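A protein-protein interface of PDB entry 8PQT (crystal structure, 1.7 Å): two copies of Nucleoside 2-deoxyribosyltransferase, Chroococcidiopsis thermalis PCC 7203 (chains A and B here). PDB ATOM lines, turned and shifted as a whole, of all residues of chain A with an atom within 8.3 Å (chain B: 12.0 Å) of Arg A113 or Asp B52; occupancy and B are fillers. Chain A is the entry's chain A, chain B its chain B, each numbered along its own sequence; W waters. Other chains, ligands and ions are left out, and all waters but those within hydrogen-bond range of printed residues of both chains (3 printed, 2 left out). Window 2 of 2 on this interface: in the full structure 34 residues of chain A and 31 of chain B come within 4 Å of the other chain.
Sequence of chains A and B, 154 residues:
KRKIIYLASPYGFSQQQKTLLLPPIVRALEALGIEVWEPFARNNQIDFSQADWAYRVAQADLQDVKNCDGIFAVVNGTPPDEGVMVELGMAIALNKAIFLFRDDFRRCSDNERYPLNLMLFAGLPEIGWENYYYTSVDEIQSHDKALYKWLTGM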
ATOM      1  N   ARG A 107     -17.384 -27.696 -33.064  1.00  0.00           N
ATOM      2  CA  ARG A 107     -18.273 -27.962 -31.943  1.00  0.00           C
ATOM      3  C   ARG A 107     -18.105 -29.423 -31.555  1.00  0.00           C
ATOM      4  O   ARG A 107     -18.021 -30.292 -32.422  1.00  0.00           O
ATOM      5  CB  ARG A 107     -19.724 -27.657 -32.308  1.00  0.00           C
ATOM      6  CG  ARG A 107     -20.029 -26.157 -32.390  1.00  0.00           C
ATOM      7  CD  ARG A 107     -21.525 -25.905 -32.631  1.00  0.00           C
ATOM      8  NE  ARG A 107     -22.332 -26.145 -31.431  1.00  0.00           N
ATOM      9  CZ  ARG A 107     -23.164 -27.167 -31.252  1.00  0.00           C
ATOM     10  NH1 ARG A 107     -23.334 -28.101 -32.178  1.00  0.00           N
ATOM     11  NH2 ARG A 107     -23.833 -27.261 -30.105  1.00  0.00           N
ATOM     12  N   SER A 109     -20.073 -31.389 -28.719  1.00  0.00           N
ATOM     13  CA  SER A 109     -21.104 -31.079 -27.733  1.00  0.00           C
ATOM     14  C   SER A 109     -22.164 -32.171 -27.622  1.00  0.00           C
ATOM     15  O   SER A 109     -22.425 -32.918 -28.564  1.00  0.00           O
ATOM     16  CB  SER A 109     -21.838 -29.786 -28.079  1.00  0.00           C
ATOM     17  OG  SER A 109     -22.702 -29.418 -27.020  1.00  0.00           O
ATOM     18  N   ASP A 110     -22.828 -32.168 -26.463  1.00  0.00           N
ATOM     19  CA  ASP A 110     -23.961 -33.026 -26.151  1.00  0.00           C
ATOM     20  C   ASP A 110     -25.271 -32.246 -26.052  1.00  0.00           C
ATOM     21  O   ASP A 110     -26.247 -32.765 -25.509  1.00  0.00           O
ATOM     22  CB  ASP A 110     -23.701 -33.783 -24.841  1.00  0.00           C
ATOM     23  CG  ASP A 110     -23.601 -32.881 -23.627  1.00  0.00           C
ATOM     24  OD1 ASP A 110     -23.442 -31.633 -23.726  1.00  0.00           O
ATOM     25  OD2 ASP A 110     -23.673 -33.453 -22.528  1.00  0.00           O
ATOM     26  N   ASN A 111     -25.328 -31.021 -26.575  1.00  0.00           N
ATOM     27  CA  ASN A 111     -26.500 -30.180 -26.358  1.00  0.00           C
ATOM     28  C   ASN A 111     -26.519 -29.036 -27.367  1.00  0.00           C
ATOM     29  O   ASN A 111     -25.532 -28.777 -28.060  1.00  0.00           O
ATOM     30  CB  ASN A 111     -26.509 -29.637 -24.935  1.00  0.00           C
ATOM     31  CG  ASN A 111     -25.430 -28.583 -24.698  1.00  0.00           C
ATOM     32  OD1 ASN A 111     -25.706 -27.368 -24.733  1.00  0.00           O
ATOM     33  ND2 ASN A 111     -24.189 -29.043 -24.452  1.00  0.00           N
ATOM     34  N   GLU A 112     -27.655 -28.325 -27.421  1.00  0.00           N
ATOM     35  CA  GLU A 112     -27.833 -27.246 -28.396  1.00  0.00           C
ATOM     36  C   GLU A 112     -27.502 -25.856 -27.845  1.00  0.00           C
ATOM     37  O   GLU A 112     -27.355 -24.921 -28.627  1.00  0.00           O
ATOM     38  CB  GLU A 112     -29.277 -27.238 -28.943  1.00  0.00           C
ATOM     39  CG  GLU A 112     -29.969 -28.613 -29.046  1.00  0.00           C
ATOM     40  CD  GLU A 112     -30.596 -29.090 -27.729  1.00  0.00           C
ATOM     41  OE1 GLU A 112     -29.871 -29.653 -26.870  1.00  0.00           O
ATOM     42  OE2 GLU A 112     -31.823 -28.896 -27.553  1.00  0.00           O
ATOM     43  N   ARG A 113     -27.368 -25.702 -26.535  1.00  0.00           N
ATOM     44  CA  ARG A 113     -27.119 -24.392 -25.939  1.00  0.00           C
ATOM     45  C   ARG A 113     -25.654 -23.984 -26.044  1.00  0.00           C
ATOM     46  O   ARG A 113     -25.345 -22.823 -26.353  1.00  0.00           O
ATOM     47  CB  ARG A 113     -27.564 -24.431 -24.477  1.00  0.00           C
ATOM     48  CG  ARG A 113     -27.119 -23.269 -23.553  1.00  0.00           C
ATOM     49  CD  ARG A 113     -27.874 -21.954 -23.696  1.00  0.00           C
ATOM     50  NE  ARG A 113     -29.310 -22.118 -23.886  1.00  0.00           N
ATOM     51  CZ  ARG A 113     -30.235 -21.859 -22.968  1.00  0.00           C
ATOM     52  NH1 ARG A 113     -29.915 -21.594 -21.710  1.00  0.00           N
ATOM     53  NH2 ARG A 113     -31.517 -21.885 -23.319  1.00  0.00           N
ATOM     54  N   TYR A 114     -24.744 -24.919 -25.775  1.00  0.00           N
ATOM     55  CA  TYR A 114     -23.333 -24.636 -25.614  1.00  0.00           C
ATOM     56  C   TYR A 114     -22.548 -25.338 -26.713  1.00  0.00           C
ATOM     57  O   TYR A 114     -22.959 -26.408 -27.183  1.00  0.00           O
ATOM     58  CB  TYR A 114     -22.804 -25.128 -24.266  1.00  0.00           C
ATOM     59  CG  TYR A 114     -23.484 -24.628 -23.017  1.00  0.00           C
ATOM     60  CD1 TYR A 114     -23.223 -23.353 -22.514  1.00  0.00           C
ATOM     61  CD2 TYR A 114     -24.366 -25.436 -22.316  1.00  0.00           C
ATOM     62  CE1 TYR A 114     -23.814 -22.905 -21.347  1.00  0.00           C
ATOM     63  CE2 TYR A 114     -24.964 -24.995 -21.142  1.00  0.00           C
ATOM     64  CZ  TYR A 114     -24.681 -23.733 -20.662  1.00  0.00           C
ATOM     65  OH  TYR A 114     -25.251 -23.285 -19.511  1.00  0.00           O
ATOM     66  N   PRO A 115     -21.413 -24.773 -27.137  1.00  0.00           N
ATOM     67  CA  PRO A 115     -20.584 -25.416 -28.166  1.00  0.00           C
ATOM     68  C   PRO A 115     -19.767 -26.590 -27.657  1.00  0.00           C
ATOM     69  O   PRO A 115     -19.073 -27.260 -28.443  1.00  0.00           O
ATOM     70  CB  PRO A 115     -19.665 -24.251 -28.606  1.00  0.00           C
ATOM     71  CG  PRO A 115     -19.492 -23.469 -27.364  1.00  0.00           C
ATOM     72  CD  PRO A 115     -20.884 -23.444 -26.782  1.00  0.00           C
ATOM     73  N   LEU A 116     -19.808 -26.845 -26.363  1.00  0.00           N
ATOM     74  CA  LEU A 116     -19.089 -27.937 -25.736  1.00  0.00           C
ATOM     75  C   LEU A 116     -20.021 -28.662 -24.767  1.00  0.00           C
ATOM     76  O   LEU A 116     -21.131 -28.207 -24.491  1.00  0.00           O
ATOM     77  CB  LEU A 116     -17.866 -27.440 -24.960  1.00  0.00           C
ATOM     78  CG  LEU A 116     -16.857 -26.641 -25.796  1.00  0.00           C
ATOM     79  CD1 LEU A 116     -15.895 -25.910 -24.864  1.00  0.00           C
ATOM     80  CD2 LEU A 116     -16.162 -27.596 -26.689  1.00  0.00           C
ATOM     81  N   LEU A 118     -22.043 -29.647 -21.796  1.00  0.00           N
ATOM     82  CA  LEU A 118     -22.685 -28.695 -20.897  1.00  0.00           C
ATOM     83  C   LEU A 118     -22.038 -28.641 -19.530  1.00  0.00           C
ATOM     84  O   LEU A 118     -22.204 -27.652 -18.815  1.00  0.00           O
ATOM     85  CB  LEU A 118     -24.176 -29.019 -20.729  1.00  0.00           C
ATOM     86  CG  LEU A 118     -24.567 -30.443 -20.289  1.00  0.00           C
ATOM     87  CD1 LEU A 118     -24.677 -30.511 -18.777  1.00  0.00           C
ATOM     88  CD2 LEU A 118     -25.883 -30.962 -20.917  1.00  0.00           C
ATOM     89  N   PHE A 121     -19.787 -25.637 -18.284  1.00  0.00           N
ATOM     90  CA  PHE A 121     -20.408 -24.345 -18.010  1.00  0.00           C
ATOM     91  C   PHE A 121     -21.150 -24.337 -16.695  1.00  0.00           C
ATOM     92  O   PHE A 121     -21.845 -23.366 -16.391  1.00  0.00           O
ATOM     93  CB  PHE A 121     -21.337 -23.986 -19.162  1.00  0.00           C
ATOM     94  CG  PHE A 121     -20.656 -24.016 -20.493  1.00  0.00           C
ATOM     95  CD1 PHE A 121     -20.519 -25.202 -21.195  1.00  0.00           C
ATOM     96  CD2 PHE A 121     -20.084 -22.852 -21.020  1.00  0.00           C
ATOM     97  CE1 PHE A 121     -19.859 -25.243 -22.417  1.00  0.00           C
ATOM     98  CE2 PHE A 121     -19.447 -22.879 -22.239  1.00  0.00           C
ATOM     99  CZ  PHE A 121     -19.321 -24.093 -22.936  1.00  0.00           C
ATOM    100  N   PRO A 125     -22.963 -18.550 -15.041  1.00  0.00           N
ATOM    101  CA  PRO A 125     -24.401 -18.288 -14.907  1.00  0.00           C
ATOM    102  C   PRO A 125     -25.196 -18.869 -16.059  1.00  0.00           C
ATOM    103  O   PRO A 125     -24.695 -19.099 -17.165  1.00  0.00           O
ATOM    104  CB  PRO A 125     -24.493 -16.752 -14.887  1.00  0.00           C
ATOM    105  CG  PRO A 125     -23.288 -16.303 -15.606  1.00  0.00           C
ATOM    106  CD  PRO A 125     -22.196 -17.313 -15.261  1.00  0.00           C
ATOM    107  N   GLU A 126     -26.470 -19.124 -15.777  1.00  0.00           N
ATOM    108  CA  GLU A 126     -27.358 -19.639 -16.806  1.00  0.00           C
ATOM    109  C   GLU A 126     -27.486 -18.653 -17.957  1.00  0.00           C
ATOM    110  O   GLU A 126     -27.488 -19.042 -19.129  1.00  0.00           O
ATOM    111  CB  GLU A 126     -28.732 -19.928 -16.206  1.00  0.00           C
ATOM    112  CG  GLU A 126     -29.722 -20.435 -17.199  1.00  0.00           C
ATOM    113  CD  GLU A 126     -31.079 -20.655 -16.579  1.00  0.00           C
ATOM    114  OE1 GLU A 126     -31.203 -20.537 -15.330  1.00  0.00           O
ATOM    115  OE2 GLU A 126     -32.010 -20.939 -17.354  1.00  0.00           O
ATOM    116  N   ILE A 127     -27.633 -17.376 -17.629  1.00  0.00           N
ATOM    117  CA  ILE A 127     -27.786 -16.306 -18.612  1.00  0.00           C
ATOM    118  C   ILE A 127     -26.522 -15.453 -18.570  1.00  0.00           C
ATOM    119  O   ILE A 127     -26.083 -15.048 -17.497  1.00  0.00           O
ATOM    120  CB  ILE A 127     -29.038 -15.460 -18.316  1.00  0.00           C
ATOM    121  CG1 ILE A 127     -30.279 -16.346 -18.201  1.00  0.00           C
ATOM    122  CG2 ILE A 127     -29.217 -14.401 -19.400  1.00  0.00           C
ATOM    123  CD1 ILE A 127     -30.526 -17.213 -19.419  1.00  0.00           C
ATOM    124  N   GLY A 128     -25.942 -15.188 -19.733  1.00  0.00           N
ATOM    125  CA  GLY A 128     -24.744 -14.365 -19.794  1.00  0.00           C
ATOM    126  C   GLY A 128     -23.433 -15.110 -19.633  1.00  0.00           C
ATOM    127  O   GLY A 128     -22.402 -14.473 -19.373  1.00  0.00           O
ATOM    128  N   TRP A 129     -23.436 -16.453 -19.759  1.00  0.00           N
ATOM    129  CA  TRP A 129     -22.179 -17.192 -19.698  1.00  0.00           C
ATOM    130  C   TRP A 129     -21.240 -16.765 -20.814  1.00  0.00           C
ATOM    131  O   TRP A 129     -20.021 -16.872 -20.669  1.00  0.00           O
ATOM    132  CB  TRP A 129     -22.425 -18.723 -19.782  1.00  0.00           C
ATOM    133  CG  TRP A 129     -23.183 -19.112 -21.001  1.00  0.00           C
ATOM    134  CD1 TRP A 129     -24.547 -19.198 -21.126  1.00  0.00           C
ATOM    135  CD2 TRP A 129     -22.650 -19.475 -22.276  1.00  0.00           C
ATOM    136  NE1 TRP A 129     -24.887 -19.579 -22.395  1.00  0.00           N
ATOM    137  CE2 TRP A 129     -23.745 -19.757 -23.125  1.00  0.00           C
ATOM    138  CE3 TRP A 129     -21.358 -19.581 -22.792  1.00  0.00           C
ATOM    139  CZ2 TRP A 129     -23.581 -20.126 -24.454  1.00  0.00           C
ATOM    140  CZ3 TRP A 129     -21.209 -19.948 -24.095  1.00  0.00           C
ATOM    141  CH2 TRP A 129     -22.306 -20.227 -24.908  1.00  0.00           C
ATOM    142  N   GLU A 130     -21.778 -16.323 -21.939  1.00  0.00           N
ATOM    143  CA  GLU A 130     -20.938 -15.924 -23.065  1.00  0.00           C
ATOM    144  C   GLU A 130     -19.968 -14.805 -22.686  1.00  0.00           C
ATOM    145  O   GLU A 130     -18.923 -14.653 -23.327  1.00  0.00           O
ATOM    146  CB  GLU A 130     -21.828 -15.468 -24.227  1.00  0.00           C
ATOM    147  CG  GLU A 130     -22.703 -16.547 -24.831  1.00  0.00           C
ATOM    148  CD  GLU A 130     -24.111 -16.546 -24.266  1.00  0.00           C
ATOM    149  OE1 GLU A 130     -24.310 -16.126 -23.099  1.00  0.00           O
ATOM    150  OE2 GLU A 130     -25.018 -16.978 -25.006  1.00  0.00           O
ATOM    151  N   ASN B  43     -31.012 -37.965 -14.551  1.00  0.00           N
ATOM    152  CA  ASN B  43     -31.564 -36.897 -15.384  1.00  0.00           C
ATOM    153  C   ASN B  43     -32.727 -37.479 -16.180  1.00  0.00           C
ATOM    154  O   ASN B  43     -32.927 -37.124 -17.336  1.00  0.00           O
ATOM    155  CB  ASN B  43     -30.549 -36.268 -16.361  1.00  0.00           C
ATOM    156  CG  ASN B  43     -29.161 -36.044 -15.758  1.00  0.00           C
ATOM    157  OD1 ASN B  43     -29.007 -35.687 -14.590  1.00  0.00           O
ATOM    158  ND2 ASN B  43     -28.139 -36.210 -16.595  1.00  0.00           N
ATOM    159  N   ASP B  52     -33.172 -23.451 -19.071  1.00  0.00           N
ATOM    160  CA  ASP B  52     -33.329 -24.524 -20.045  1.00  0.00           C
ATOM    161  C   ASP B  52     -32.618 -25.817 -19.612  1.00  0.00           C
ATOM    162  O   ASP B  52     -31.927 -25.870 -18.575  1.00  0.00           O
ATOM    163  CB  ASP B  52     -32.817 -24.070 -21.409  1.00  0.00           C
ATOM    164  CG  ASP B  52     -33.548 -24.728 -22.557  1.00  0.00           C
ATOM    165  OD1 ASP B  52     -34.799 -24.744 -22.551  1.00  0.00           O
ATOM    166  OD2 ASP B  52     -32.864 -25.219 -23.476  1.00  0.00           O
ATOM    167  N   TRP B  53     -32.786 -26.859 -20.432  1.00  0.00           N
ATOM    168  CA  TRP B  53     -32.540 -28.208 -19.940  1.00  0.00           C
ATOM    169  C   TRP B  53     -31.055 -28.453 -19.726  1.00  0.00           C
ATOM    170  O   TRP B  53     -30.664 -29.097 -18.748  1.00  0.00           O
ATOM    171  CB  TRP B  53     -33.164 -29.229 -20.894  1.00  0.00           C
ATOM    172  CG  TRP B  53     -32.462 -29.498 -22.201  1.00  0.00           C
ATOM    173  CD1 TRP B  53     -32.839 -29.060 -23.445  1.00  0.00           C
ATOM    174  CD2 TRP B  53     -31.313 -30.342 -22.408  1.00  0.00           C
ATOM    175  NE1 TRP B  53     -31.980 -29.552 -24.402  1.00  0.00           N
ATOM    176  CE2 TRP B  53     -31.039 -30.343 -23.794  1.00  0.00           C
ATOM    177  CE3 TRP B  53     -30.488 -31.087 -21.558  1.00  0.00           C
ATOM    178  CZ2 TRP B  53     -29.972 -31.056 -24.342  1.00  0.00           C
ATOM    179  CZ3 TRP B  53     -29.425 -31.794 -22.110  1.00  0.00           C
ATOM    180  CH2 TRP B  53     -29.181 -31.775 -23.482  1.00  0.00           C
ATOM    181  N   ALA B  54     -30.203 -27.887 -20.585  1.00  0.00           N
ATOM    182  CA  ALA B  54     -28.776 -28.173 -20.469  1.00  0.00           C
ATOM    183  C   ALA B  54     -28.205 -27.613 -19.176  1.00  0.00           C
ATOM    184  O   ALA B  54     -27.432 -28.292 -18.486  1.00  0.00           O
ATOM    185  CB  ALA B  54     -28.036 -27.628 -21.696  1.00  0.00           C
ATOM    186  N   TYR B  55     -28.583 -26.382 -18.810  1.00  0.00           N
ATOM    187  CA  TYR B  55     -28.099 -25.817 -17.557  1.00  0.00           C
ATOM    188  C   TYR B  55     -28.606 -26.619 -16.365  1.00  0.00           C
ATOM    189  O   TYR B  55     -27.875 -26.830 -15.392  1.00  0.00           O
ATOM    190  CB  TYR B  55     -28.538 -24.353 -17.443  1.00  0.00           C
ATOM    191  CG  TYR B  55     -28.090 -23.700 -16.175  1.00  0.00           C
ATOM    192  CD1 TYR B  55     -26.801 -23.202 -16.039  1.00  0.00           C
ATOM    193  CD2 TYR B  55     -28.966 -23.561 -15.105  1.00  0.00           C
ATOM    194  CE1 TYR B  55     -26.384 -22.616 -14.867  1.00  0.00           C
ATOM    195  CE2 TYR B  55     -28.558 -22.965 -13.925  1.00  0.00           C
ATOM    196  CZ  TYR B  55     -27.267 -22.495 -13.813  1.00  0.00           C
ATOM    197  OH  TYR B  55     -26.873 -21.920 -12.629  1.00  0.00           O
ATOM    198  N   ARG B  56     -29.860 -27.073 -16.435  1.00  0.00           N
ATOM    199  CA  ARG B  56     -30.427 -27.866 -15.351  1.00  0.00           C
ATOM    200  C   ARG B  56     -29.686 -29.190 -15.183  1.00  0.00           C
ATOM    201  O   ARG B  56     -29.473 -29.640 -14.052  1.00  0.00           O
ATOM    202  CB  ARG B  56     -31.923 -28.088 -15.619  1.00  0.00           C
ATOM    203  CG  ARG B  56     -32.786 -26.833 -15.348  1.00  0.00           C
ATOM    204  CD  ARG B  56     -34.259 -27.169 -15.123  1.00  0.00           C
ATOM    205  NE  ARG B  56     -35.099 -25.976 -15.111  1.00  0.00           N
ATOM    206  CZ  ARG B  56     -35.689 -25.470 -14.033  1.00  0.00           C
ATOM    207  NH1 ARG B  56     -35.545 -26.020 -12.837  1.00  0.00           N
ATOM    208  NH2 ARG B  56     -36.436 -24.376 -14.157  1.00  0.00           N
ATOM    209  N   VAL B  57     -29.290 -29.835 -16.289  1.00  0.00           N
ATOM    210  CA  VAL B  57     -28.541 -31.090 -16.155  1.00  0.00           C
ATOM    211  C   VAL B  57     -27.210 -30.816 -15.469  1.00  0.00           C
ATOM    212  O   VAL B  57     -26.774 -31.543 -14.565  1.00  0.00           O
ATOM    213  CB  VAL B  57     -28.319 -31.751 -17.528  1.00  0.00           C
ATOM    214  CG1 VAL B  57     -27.245 -32.891 -17.409  1.00  0.00           C
ATOM    215  CG2 VAL B  57     -29.614 -32.253 -18.137  1.00  0.00           C
ATOM    216  N   ALA B  58     -26.540 -29.750 -15.894  1.00  0.00           N
ATOM    217  CA  ALA B  58     -25.267 -29.386 -15.291  1.00  0.00           C
ATOM    218  C   ALA B  58     -25.393 -29.158 -13.790  1.00  0.00           C
ATOM    219  O   ALA B  58     -24.553 -29.640 -13.011  1.00  0.00           O
ATOM    220  CB  ALA B  58     -24.702 -28.149 -16.000  1.00  0.00           C
ATOM    221  N   GLN B  59     -26.441 -28.445 -13.356  1.00  0.00           N
ATOM    222  CA  GLN B  59     -26.583 -28.172 -11.929  1.00  0.00           C
ATOM    223  C   GLN B  59     -26.957 -29.439 -11.148  1.00  0.00           C
ATOM    224  O   GLN B  59     -26.511 -29.616 -10.012  1.00  0.00           O
ATOM    225  CB  GLN B  59     -27.621 -27.079 -11.695  1.00  0.00           C
ATOM    226  CG  GLN B  59     -27.221 -25.701 -12.252  1.00  0.00           C
ATOM    227  CD  GLN B  59     -25.821 -25.282 -11.844  1.00  0.00           C
ATOM    228  OE1 GLN B  59     -25.505 -25.197 -10.666  1.00  0.00           O
ATOM    229  NE2 GLN B  59     -24.972 -25.029 -12.828  1.00  0.00           N
ATOM    230  N   ALA B  60     -27.782 -30.302 -11.736  1.00  0.00           N
ATOM    231  CA  ALA B  60     -28.137 -31.570 -11.101  1.00  0.00           C
ATOM    232  C   ALA B  60     -26.906 -32.440 -10.895  1.00  0.00           C
ATOM    233  O   ALA B  60     -26.698 -32.993  -9.811  1.00  0.00           O
ATOM    234  CB  ALA B  60     -29.164 -32.302 -11.957  1.00  0.00           C
ATOM    235  N   ASP B  61     -26.070 -32.576 -11.932  1.00  0.00           N
ATOM    236  CA  ASP B  61     -24.853 -33.362 -11.780  1.00  0.00           C
ATOM    237  C   ASP B  61     -23.934 -32.751 -10.731  1.00  0.00           C
ATOM    238  O   ASP B  61     -23.336 -33.469  -9.925  1.00  0.00           O
ATOM    239  CB  ASP B  61     -24.121 -33.478 -13.117  1.00  0.00           C
ATOM    240  CG  ASP B  61     -24.860 -34.345 -14.132  1.00  0.00           C
ATOM    241  OD1 ASP B  61     -25.895 -34.939 -13.770  1.00  0.00           O
ATOM    242  OD2 ASP B  61     -24.403 -34.432 -15.312  1.00  0.00           O
HETATM  243  O   HOH W   1     -27.634 -18.585 -13.079  1.00  0.00           O
HETATM  244  O   HOH W   2     -34.166 -29.147 -26.241  1.00  0.00           O
HETATM  245  O   HOH W   3     -31.938 -20.515 -20.490  1.00  0.00           O
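Asn A111 touches just these residues of chain B: Trp B53 (3.7 Å) and Ala B54 (3.8 Å). Of chain B, only Trp B53 comes within 4 Å of Glu A112. Arg A113 touches just one residue of chain B: Asp B52 (3.2 Å). Tyr A114 touches one residue of chain B. No residue of chain B comes within 4 Å of Pro A115. Of the printed residues of chain B, Leu A118 touches Trp B53, Ala B54, Val B57 and Ala B58. Glu A126 touches just these residues of chain B: Asp B52 and Tyr B55. Asp B52 touches just these residues of chain A: Arg A113 (3.2 Å) and Glu A126 (3.3 Å). Printed residues of chain A within 4 Å of Ala B54: Asn A111 (3.8 Å) and Leu A118 (3.5 Å). Of the printed residues of chain A, Val B57 touches Leu A118 (3.8 Å). Of the printed residues of chain A, Ala B58 touches Leu A118 (3.5 Å). The nearest residue of chain B that does not touch Arg A113 is Ala B54 (4.3 Å). The nearest printed residue of chain A that does not touch Ala B54 is Tyr A114 (4.1 Å).
The side-chain amide oxygen (OD1) of Asn A111 is in hydrogen-bond range of the backbone NH (N) of Arg A113 (3.0 Å). NH2 of Arg A107 is in hydrogen-bond range of O of Asn A111, 3.1 Å away. The guanidinium group (NH2) of Arg A107 sits at hydrogen-bond distance from the backbone carbonyl oxygen (O) of Tyr A114 (3.2 Å). The side-chain carboxylate (OD1) of Asp A110 lies within hydrogen-bond range of the side-chain amide nitrogen (ND2) of Asn A111, 2.8 Å away. The side-chain amide nitrogen of Asn A111 is in hydrogen-bond range of the backbone carbonyl oxygen of Leu A116 (3.2 Å). The backbone NH (N) of Leu A118 lies within hydrogen-bond range of the side-chain carboxylate (OD1) of Asp A110.
Of the 17 printed residues of chain A, 7 touch a printed residue of chain B. Hydrophobic or aromatic side chains of chain A that line the printed part of chain B: Tyr A114 and Leu A118. Along chain A the printed residues that touch a printed residue of chain B span positions 110 to 126. Printed residues of chain B that touch a printed residue of chain A: Asp B52, Trp B53, Ala B54, Tyr B55, Val B57 and Ala B58. Hydrophobic or aromatic side chains of chain B that line the printed part of chain A: Trp B53, Ala B54, Tyr B55, Val B57 and Ala B58. Among the printed residues, 12 pairs touch across the chains.
OD2 of Asp B52 is in salt-bridge range of NH2 of Arg A113, 3.6 Å away. The side-chain carboxylate (OE2) of Glu A126 sits at hydrogen-bond distance from the backbone NH (N) of Asp B52, 3.3 Å away. The side-chain carboxylate of Glu A112 lies within hydrogen-bond range of the indole nitrogen of Trp B53.
Among the printed residues, pairs that only touch across the chains: Leu A118 with Ala B58 (3.5 Å), Leu A118 with Ala B54 (3.5 Å), Glu A126 with Tyr B55 (3.6 Å), Asp A110 with Trp B53 (3.7 Å), Asn A111 with Trp B53 (3.7 Å), Leu A118 with Val B57 (3.8 Å), Tyr A114 with Tyr B55 (3.8 Å), Leu A118 with Trp B53 (3.8 Å) and Asn A111 with Ala B54 (3.8 Å).
Water W3 lies within hydrogen-bond range of the guanidinium group (NH1) of Arg A113, the side-chain carboxylate (OE2) of Glu A126 and the backbone NH (N) of Asp B52. Water W2 lies within hydrogen-bond range of the side-chain carboxylate of Glu A112 (2.7 Å) and the indole nitrogen of Trp B53 (2.9 Å). Water W1 lies within hydrogen-bond range of N of Glu A126 (3.0 Å) and OH of Tyr B55 (3.5 Å).
No position is printed for both chains. Of the 12 pairs that touch across the chains among the printed residues, none has its exchanged pair printed and touching as well.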
